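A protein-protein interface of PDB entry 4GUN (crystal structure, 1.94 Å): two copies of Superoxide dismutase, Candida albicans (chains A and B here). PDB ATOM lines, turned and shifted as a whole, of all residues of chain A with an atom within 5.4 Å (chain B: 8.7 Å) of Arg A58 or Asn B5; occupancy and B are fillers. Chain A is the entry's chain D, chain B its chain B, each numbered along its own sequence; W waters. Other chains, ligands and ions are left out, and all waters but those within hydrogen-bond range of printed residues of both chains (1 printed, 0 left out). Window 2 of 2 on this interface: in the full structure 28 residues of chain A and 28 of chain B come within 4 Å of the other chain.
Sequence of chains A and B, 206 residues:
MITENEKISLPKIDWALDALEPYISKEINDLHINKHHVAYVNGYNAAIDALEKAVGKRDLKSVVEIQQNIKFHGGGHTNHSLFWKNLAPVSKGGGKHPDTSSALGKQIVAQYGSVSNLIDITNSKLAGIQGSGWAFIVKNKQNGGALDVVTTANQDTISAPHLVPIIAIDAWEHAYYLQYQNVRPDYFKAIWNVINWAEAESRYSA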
ATOM      1  N   ALA A  54       5.559  24.521  -8.678  1.00  0.00           N
ATOM      2  CA  ALA A  54       5.852  23.384  -7.797  1.00  0.00           C
ATOM      3  C   ALA A  54       7.089  23.589  -6.868  1.00  0.00           C
ATOM      4  O   ALA A  54       7.037  23.192  -5.694  1.00  0.00           O
ATOM      5  CB  ALA A  54       6.001  22.106  -8.616  1.00  0.00           C
ATOM      6  N   VAL A  55       8.192  24.185  -7.396  1.00  0.00           N
ATOM      7  CA  VAL A  55       9.441  24.470  -6.664  1.00  0.00           C
ATOM      8  C   VAL A  55       9.142  25.430  -5.503  1.00  0.00           C
ATOM      9  O   VAL A  55       9.572  25.187  -4.366  1.00  0.00           O
ATOM     10  CB  VAL A  55      10.591  25.000  -7.601  1.00  0.00           C
ATOM     11  CG1 VAL A  55      11.666  25.779  -6.834  1.00  0.00           C
ATOM     12  CG2 VAL A  55      11.230  23.859  -8.390  1.00  0.00           C
ATOM     13  N   GLY A  56       8.371  26.474  -5.806  1.00  0.00           N
ATOM     14  CA  GLY A  56       7.974  27.492  -4.847  1.00  0.00           C
ATOM     15  C   GLY A  56       7.222  26.939  -3.656  1.00  0.00           C
ATOM     16  O   GLY A  56       7.382  27.439  -2.539  1.00  0.00           O
ATOM     17  N   LYS A  57       6.401  25.891  -3.893  1.00  0.00           N
ATOM     18  CA  LYS A  57       5.568  25.228  -2.884  1.00  0.00           C
ATOM     19  C   LYS A  57       6.286  24.055  -2.214  1.00  0.00           C
ATOM     20  O   LYS A  57       5.701  23.411  -1.333  1.00  0.00           O
ATOM     21  CB  LYS A  57       4.262  24.716  -3.533  1.00  0.00           C
ATOM     22  CG  LYS A  57       3.350  25.803  -4.097  1.00  0.00           C
ATOM     23  CD  LYS A  57       2.099  25.177  -4.708  1.00  0.00           C
ATOM     24  CE  LYS A  57       0.959  26.158  -4.850  1.00  0.00           C
ATOM     25  NZ  LYS A  57      -0.365  25.486  -4.765  1.00  0.00           N
ATOM     26  N   ARG A  58       7.545  23.766  -2.637  1.00  0.00           N
ATOM     27  CA  ARG A  58       8.346  22.623  -2.174  1.00  0.00           C
ATOM     28  C   ARG A  58       7.570  21.321  -2.403  1.00  0.00           C
ATOM     29  O   ARG A  58       7.589  20.435  -1.544  1.00  0.00           O
ATOM     30  CB  ARG A  58       8.768  22.755  -0.692  1.00  0.00           C
ATOM     31  CG  ARG A  58      10.040  23.531  -0.435  1.00  0.00           C
ATOM     32  CD  ARG A  58      10.645  23.256   0.948  1.00  0.00           C
ATOM     33  NE  ARG A  58       9.665  23.235   2.040  1.00  0.00           N
ATOM     34  CZ  ARG A  58       9.276  24.303   2.732  1.00  0.00           C
ATOM     35  NH1 ARG A  58       9.785  25.500   2.464  1.00  0.00           N
ATOM     36  NH2 ARG A  58       8.380  24.183   3.703  1.00  0.00           N
ATOM     37  N   ASP A  59       6.847  21.224  -3.541  1.00  0.00           N
ATOM     38  CA  ASP A  59       6.053  20.049  -3.875  1.00  0.00           C
ATOM     39  C   ASP A  59       6.991  19.098  -4.621  1.00  0.00           C
ATOM     40  O   ASP A  59       6.969  19.051  -5.851  1.00  0.00           O
ATOM     41  CB  ASP A  59       4.836  20.464  -4.735  1.00  0.00           C
ATOM     42  CG  ASP A  59       3.900  19.334  -5.139  1.00  0.00           C
ATOM     43  OD1 ASP A  59       2.897  19.615  -5.836  1.00  0.00           O
ATOM     44  OD2 ASP A  59       4.163  18.168  -4.750  1.00  0.00           O
ATOM     45  N   LEU A  60       7.862  18.396  -3.870  1.00  0.00           N
ATOM     46  CA  LEU A  60       8.884  17.541  -4.464  1.00  0.00           C
ATOM     47  C   LEU A  60       8.395  16.432  -5.351  1.00  0.00           C
ATOM     48  O   LEU A  60       9.077  16.107  -6.324  1.00  0.00           O
ATOM     49  CB  LEU A  60      10.026  17.145  -3.508  1.00  0.00           C
ATOM     50  CG  LEU A  60      11.186  18.166  -3.483  1.00  0.00           C
ATOM     51  CD1 LEU A  60      10.722  19.573  -2.943  1.00  0.00           C
ATOM     52  CD2 LEU A  60      12.368  17.642  -2.703  1.00  0.00           C
ATOM     53  N   VAL A  63       7.676  18.446  -8.640  1.00  0.00           N
ATOM     54  CA  VAL A  63       9.009  18.859  -9.099  1.00  0.00           C
ATOM     55  C   VAL A  63       9.675  17.678  -9.856  1.00  0.00           C
ATOM     56  O   VAL A  63      10.090  17.831 -11.015  1.00  0.00           O
ATOM     57  CB  VAL A  63       9.871  19.376  -7.920  1.00  0.00           C
ATOM     58  CG1 VAL A  63      11.341  19.518  -8.308  1.00  0.00           C
ATOM     59  CG2 VAL A  63       9.333  20.691  -7.382  1.00  0.00           C
ATOM     60  N   ILE B   2      18.188  31.126  -5.494  1.00  0.00           N
ATOM     61  CA  ILE B   2      17.255  30.312  -4.701  1.00  0.00           C
ATOM     62  C   ILE B   2      16.696  31.099  -3.514  1.00  0.00           C
ATOM     63  O   ILE B   2      17.456  31.780  -2.833  1.00  0.00           O
ATOM     64  CB  ILE B   2      17.847  28.918  -4.300  1.00  0.00           C
ATOM     65  CG1 ILE B   2      16.757  27.981  -3.703  1.00  0.00           C
ATOM     66  CG2 ILE B   2      19.111  29.035  -3.399  1.00  0.00           C
ATOM     67  CD1 ILE B   2      17.168  26.526  -3.392  1.00  0.00           C
ATOM     68  N   THR B   3      15.374  31.003  -3.276  1.00  0.00           N
ATOM     69  CA  THR B   3      14.684  31.677  -2.164  1.00  0.00           C
ATOM     70  C   THR B   3      14.433  30.694  -0.992  1.00  0.00           C
ATOM     71  O   THR B   3      14.449  29.479  -1.201  1.00  0.00           O
ATOM     72  CB  THR B   3      13.421  32.425  -2.653  1.00  0.00           C
ATOM     73  OG1 THR B   3      12.420  31.490  -3.037  1.00  0.00           O
ATOM     74  CG2 THR B   3      13.704  33.387  -3.809  1.00  0.00           C
ATOM     75  N   GLU B   4      14.221  31.220   0.224  1.00  0.00           N
ATOM     76  CA  GLU B   4      14.005  30.458   1.464  1.00  0.00           C
ATOM     77  C   GLU B   4      12.979  29.344   1.356  1.00  0.00           C
ATOM     78  O   GLU B   4      13.253  28.212   1.750  1.00  0.00           O
ATOM     79  CB  GLU B   4      13.614  31.410   2.611  1.00  0.00           C
ATOM     80  CG  GLU B   4      13.028  30.738   3.861  1.00  0.00           C
ATOM     81  CD  GLU B   4      11.512  30.629   4.032  1.00  0.00           C
ATOM     82  OE1 GLU B   4      10.780  31.616   3.760  1.00  0.00           O
ATOM     83  OE2 GLU B   4      11.070  29.556   4.508  1.00  0.00           O
ATOM     84  N   ASN B   5      11.777  29.702   0.886  1.00  0.00           N
ATOM     85  CA  ASN B   5      10.600  28.852   0.754  1.00  0.00           C
ATOM     86  C   ASN B   5      10.827  27.629  -0.115  1.00  0.00           C
ATOM     87  O   ASN B   5      10.079  26.662   0.012  1.00  0.00           O
ATOM     88  CB  ASN B   5       9.414  29.672   0.213  1.00  0.00           C
ATOM     89  CG  ASN B   5       9.667  30.284  -1.147  1.00  0.00           C
ATOM     90  OD1 ASN B   5      10.622  31.041  -1.343  1.00  0.00           O
ATOM     91  ND2 ASN B   5       8.807  29.988  -2.114  1.00  0.00           N
ATOM     92  N   GLU B   6      11.821  27.692  -1.020  1.00  0.00           N
ATOM     93  CA  GLU B   6      12.168  26.623  -1.969  1.00  0.00           C
ATOM     94  C   GLU B   6      13.097  25.586  -1.362  1.00  0.00           C
ATOM     95  O   GLU B   6      13.099  24.437  -1.808  1.00  0.00           O
ATOM     96  CB  GLU B   6      12.830  27.215  -3.227  1.00  0.00           C
ATOM     97  CG  GLU B   6      11.998  28.282  -3.914  1.00  0.00           C
ATOM     98  CD  GLU B   6      12.586  28.904  -5.166  1.00  0.00           C
ATOM     99  OE1 GLU B   6      13.832  28.963  -5.286  1.00  0.00           O
ATOM    100  OE2 GLU B   6      11.795  29.379  -6.011  1.00  0.00           O
ATOM    101  N   LYS B   7      13.886  25.986  -0.358  1.00  0.00           N
ATOM    102  CA  LYS B   7      14.879  25.128   0.293  1.00  0.00           C
ATOM    103  C   LYS B   7      14.271  24.025   1.157  1.00  0.00           C
ATOM    104  O   LYS B   7      13.431  24.315   2.011  1.00  0.00           O
ATOM    105  CB  LYS B   7      15.857  25.970   1.145  1.00  0.00           C
ATOM    106  CG  LYS B   7      16.869  26.794   0.353  1.00  0.00           C
ATOM    107  CD  LYS B   7      17.887  27.483   1.274  1.00  0.00           C
ATOM    108  CE  LYS B   7      17.462  28.881   1.677  1.00  0.00           C
ATOM    109  NZ  LYS B   7      18.145  29.350   2.915  1.00  0.00           N
ATOM    110  N   ILE B   8      14.741  22.767   0.977  1.00  0.00           N
ATOM    111  CA  ILE B   8      14.312  21.624   1.795  1.00  0.00           C
ATOM    112  C   ILE B   8      15.251  21.432   2.997  1.00  0.00           C
ATOM    113  O   ILE B   8      16.370  21.935   2.984  1.00  0.00           O
ATOM    114  CB  ILE B   8      14.106  20.300   0.989  1.00  0.00           C
ATOM    115  CG1 ILE B   8      15.450  19.804   0.394  1.00  0.00           C
ATOM    116  CG2 ILE B   8      12.999  20.480  -0.058  1.00  0.00           C
ATOM    117  CD1 ILE B   8      15.514  18.395  -0.220  1.00  0.00           C
ATOM    118  N   SER B   9      14.805  20.675   4.009  1.00  0.00           N
ATOM    119  CA  SER B   9      15.564  20.411   5.229  1.00  0.00           C
ATOM    120  C   SER B   9      15.498  18.954   5.596  1.00  0.00           C
ATOM    121  O   SER B   9      14.574  18.243   5.194  1.00  0.00           O
ATOM    122  CB  SER B   9      14.996  21.225   6.403  1.00  0.00           C
ATOM    123  OG  SER B   9      14.888  22.603   6.089  1.00  0.00           O
ATOM    124  N   TYR B  44      19.781  18.722  -3.673  1.00  0.00           N
ATOM    125  CA  TYR B  44      18.545  19.308  -4.225  1.00  0.00           C
ATOM    126  C   TYR B  44      18.589  20.840  -4.188  1.00  0.00           C
ATOM    127  O   TYR B  44      18.252  21.494  -5.187  1.00  0.00           O
ATOM    128  CB  TYR B  44      17.302  18.785  -3.479  1.00  0.00           C
ATOM    129  CG  TYR B  44      16.002  19.432  -3.932  1.00  0.00           C
ATOM    130  CD1 TYR B  44      15.303  18.944  -5.031  1.00  0.00           C
ATOM    131  CD2 TYR B  44      15.487  20.547  -3.274  1.00  0.00           C
ATOM    132  CE1 TYR B  44      14.112  19.534  -5.454  1.00  0.00           C
ATOM    133  CE2 TYR B  44      14.313  21.165  -3.706  1.00  0.00           C
ATOM    134  CZ  TYR B  44      13.626  20.654  -4.798  1.00  0.00           C
ATOM    135  OH  TYR B  44      12.471  21.260  -5.245  1.00  0.00           O
ATOM    136  N   ASN B  45      18.978  21.412  -3.023  1.00  0.00           N
ATOM    137  CA  ASN B  45      19.050  22.867  -2.864  1.00  0.00           C
ATOM    138  C   ASN B  45      20.059  23.490  -3.824  1.00  0.00           C
ATOM    139  O   ASN B  45      19.762  24.522  -4.430  1.00  0.00           O
ATOM    140  CB  ASN B  45      19.305  23.247  -1.410  1.00  0.00           C
ATOM    141  CG  ASN B  45      18.204  22.836  -0.458  1.00  0.00           C
ATOM    142  OD1 ASN B  45      17.018  22.815  -0.789  1.00  0.00           O
ATOM    143  ND2 ASN B  45      18.565  22.562   0.776  1.00  0.00           N
ATOM    144  N   ILE B  48      18.394  23.219  -7.529  1.00  0.00           N
ATOM    145  CA  ILE B  48      17.349  24.237  -7.706  1.00  0.00           C
ATOM    146  C   ILE B  48      17.999  25.593  -7.991  1.00  0.00           C
ATOM    147  O   ILE B  48      17.558  26.301  -8.891  1.00  0.00           O
ATOM    148  CB  ILE B  48      16.350  24.249  -6.500  1.00  0.00           C
ATOM    149  CG1 ILE B  48      15.484  22.982  -6.497  1.00  0.00           C
ATOM    150  CG2 ILE B  48      15.460  25.512  -6.444  1.00  0.00           C
ATOM    151  CD1 ILE B  48      14.674  22.636  -7.798  1.00  0.00           C
ATOM    152  N   GLU B  52      17.574  27.550 -11.695  1.00  0.00           N
ATOM    153  CA  GLU B  52      16.995  28.884 -11.809  1.00  0.00           C
ATOM    154  C   GLU B  52      17.897  29.835 -12.580  1.00  0.00           C
ATOM    155  O   GLU B  52      17.402  30.563 -13.432  1.00  0.00           O
ATOM    156  CB  GLU B  52      16.590  29.412 -10.431  1.00  0.00           C
ATOM    157  CG  GLU B  52      15.432  28.605  -9.856  1.00  0.00           C
ATOM    158  CD  GLU B  52      15.018  28.832  -8.414  1.00  0.00           C
ATOM    159  OE1 GLU B  52      14.004  28.222  -8.006  1.00  0.00           O
ATOM    160  OE2 GLU B  52      15.688  29.609  -7.693  1.00  0.00           O
ATOM    161  N   HIS B  77      15.461  12.754  -1.301  1.00  0.00           N
ATOM    162  CA  HIS B  77      14.842  13.332  -0.105  1.00  0.00           C
ATOM    163  C   HIS B  77      13.436  12.748   0.118  1.00  0.00           C
ATOM    164  O   HIS B  77      13.104  12.418   1.258  1.00  0.00           O
ATOM    165  CB  HIS B  77      14.786  14.860  -0.222  1.00  0.00           C
ATOM    166  CG  HIS B  77      13.970  15.521   0.844  1.00  0.00           C
ATOM    167  ND1 HIS B  77      14.417  15.599   2.148  1.00  0.00           N
ATOM    168  CD2 HIS B  77      12.777  16.150   0.749  1.00  0.00           C
ATOM    169  CE1 HIS B  77      13.477  16.250   2.815  1.00  0.00           C
ATOM    170  NE2 HIS B  77      12.477  16.618   2.014  1.00  0.00           N
ATOM    171  N   THR B  78      12.598  12.656  -0.950  1.00  0.00           N
ATOM    172  CA  THR B  78      11.216  12.132  -0.827  1.00  0.00           C
ATOM    173  C   THR B  78      11.215  10.692  -0.292  1.00  0.00           C
ATOM    174  O   THR B  78      10.491  10.382   0.651  1.00  0.00           O
ATOM    175  CB  THR B  78      10.466  12.213  -2.166  1.00  0.00           C
ATOM    176  OG1 THR B  78      10.535  13.537  -2.675  1.00  0.00           O
ATOM    177  CG2 THR B  78       9.007  11.760  -2.058  1.00  0.00           C
HETATM  178  O   HOH W   1      11.593  23.407  -3.754  1.00  0.00           O
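The backbone carbonyl oxygen (O) of Gly A56 sits at hydrogen-bond distance from the side-chain amide nitrogen (ND2) of Asn B5, at 3.0 Å. The backbone carbonyl oxygen (O) of Asn B5 is in hydrogen-bond range of the guanidinium group (NH1) of Arg A58, 2.7 Å away.
The side-chain amide oxygen of Asn B5 sits at hydrogen-bond distance from the side-chain hydroxyl of Thr B3, at 2.5 Å. The backbone NH (N) of Thr B3 sits at hydrogen-bond distance from the side-chain carboxylate (OE1) of Glu B6 (3.3 Å). The backbone NH (N) of Ile B8 sits at hydrogen-bond distance from the side-chain amide oxygen (OD1) of Asn B45 (2.9 Å).
CG1 of Val A55 touches CD of Glu B6, 3.7 Å away. OE1 of Glu B52 touches CG1 of Val A55 (3.6 Å). Glu B6 touches Arg A58 (O to CG, 3.5 Å). Arg A58 touches Lys B7 (CD to O, 3.2 Å). CG2 of Ile B8 touches CD of Arg A58 (3.8 Å). Ile B8 touches Leu A60 (CG2 to CD1, 3.8 Å). CD1 of Leu A60 touches OH of Tyr B44, 3.3 Å away. Leu A60 touches His B77 (CD2 to CD2, 3.8 Å). CB of Leu A60 touches OG1 of Thr B78 (3.7 Å). Tyr B44 touches Val A63 (OH to CG1, 3.7 Å).
Of chain B, only Asn B5 (2.7 Å), Glu B6 (3.5 Å), Lys B7 (3.2 Å) and Ile B8 (3.8 Å) come within 4 Å of Arg A58. Printed residues of chain B within 4 Å of Leu A60: Ile B8, Tyr B44, His B77 and Thr B78. Of chain A, only Gly A56 (3.0 Å) and Arg A58 (2.7 Å) come within 4 Å of Asn B5. Of the printed residues of chain A, Glu B6 touches Val A55 and Arg A58. Of the printed residues of chain A, Lys B7 touches Arg A58 (3.2 Å). Asn B45 touches none of the printed residues of chain A. Printed residues of chain A within 4 Å of Ile B48: Val A55. Printed residues of chain A within 4 Å of Thr B78: Leu A60. The nearest residue of chain A that does not touch Asn B5 is Val A55 (4.6 Å).
Hydrophobic or aromatic side chains of chain B that line the printed part of chain A: Ile B8, Tyr B44, Ile B48 and His B77. Of the 8 printed residues of chain A, 5 touch a printed residue of chain B. Hydrophobic or aromatic side chains of chain A within 4 Å of the printed part of chain B: Val A55, Leu A60 and Val A63. Along chain A the printed residues that touch a printed residue of chain B span positions 55 to 63. Among the printed residues, 13 pairs touch across the chains.
No position is printed for both chains. Of the 13 pairs that touch across the chains among the printed residues, none has its exchanged pair printed and touching as well.
Water W1 lies within hydrogen-bond range of O of Glu B6 (2.7 Å), OH of Tyr B44 (2.8 Å) and O of Val A55 (2.8 Å).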
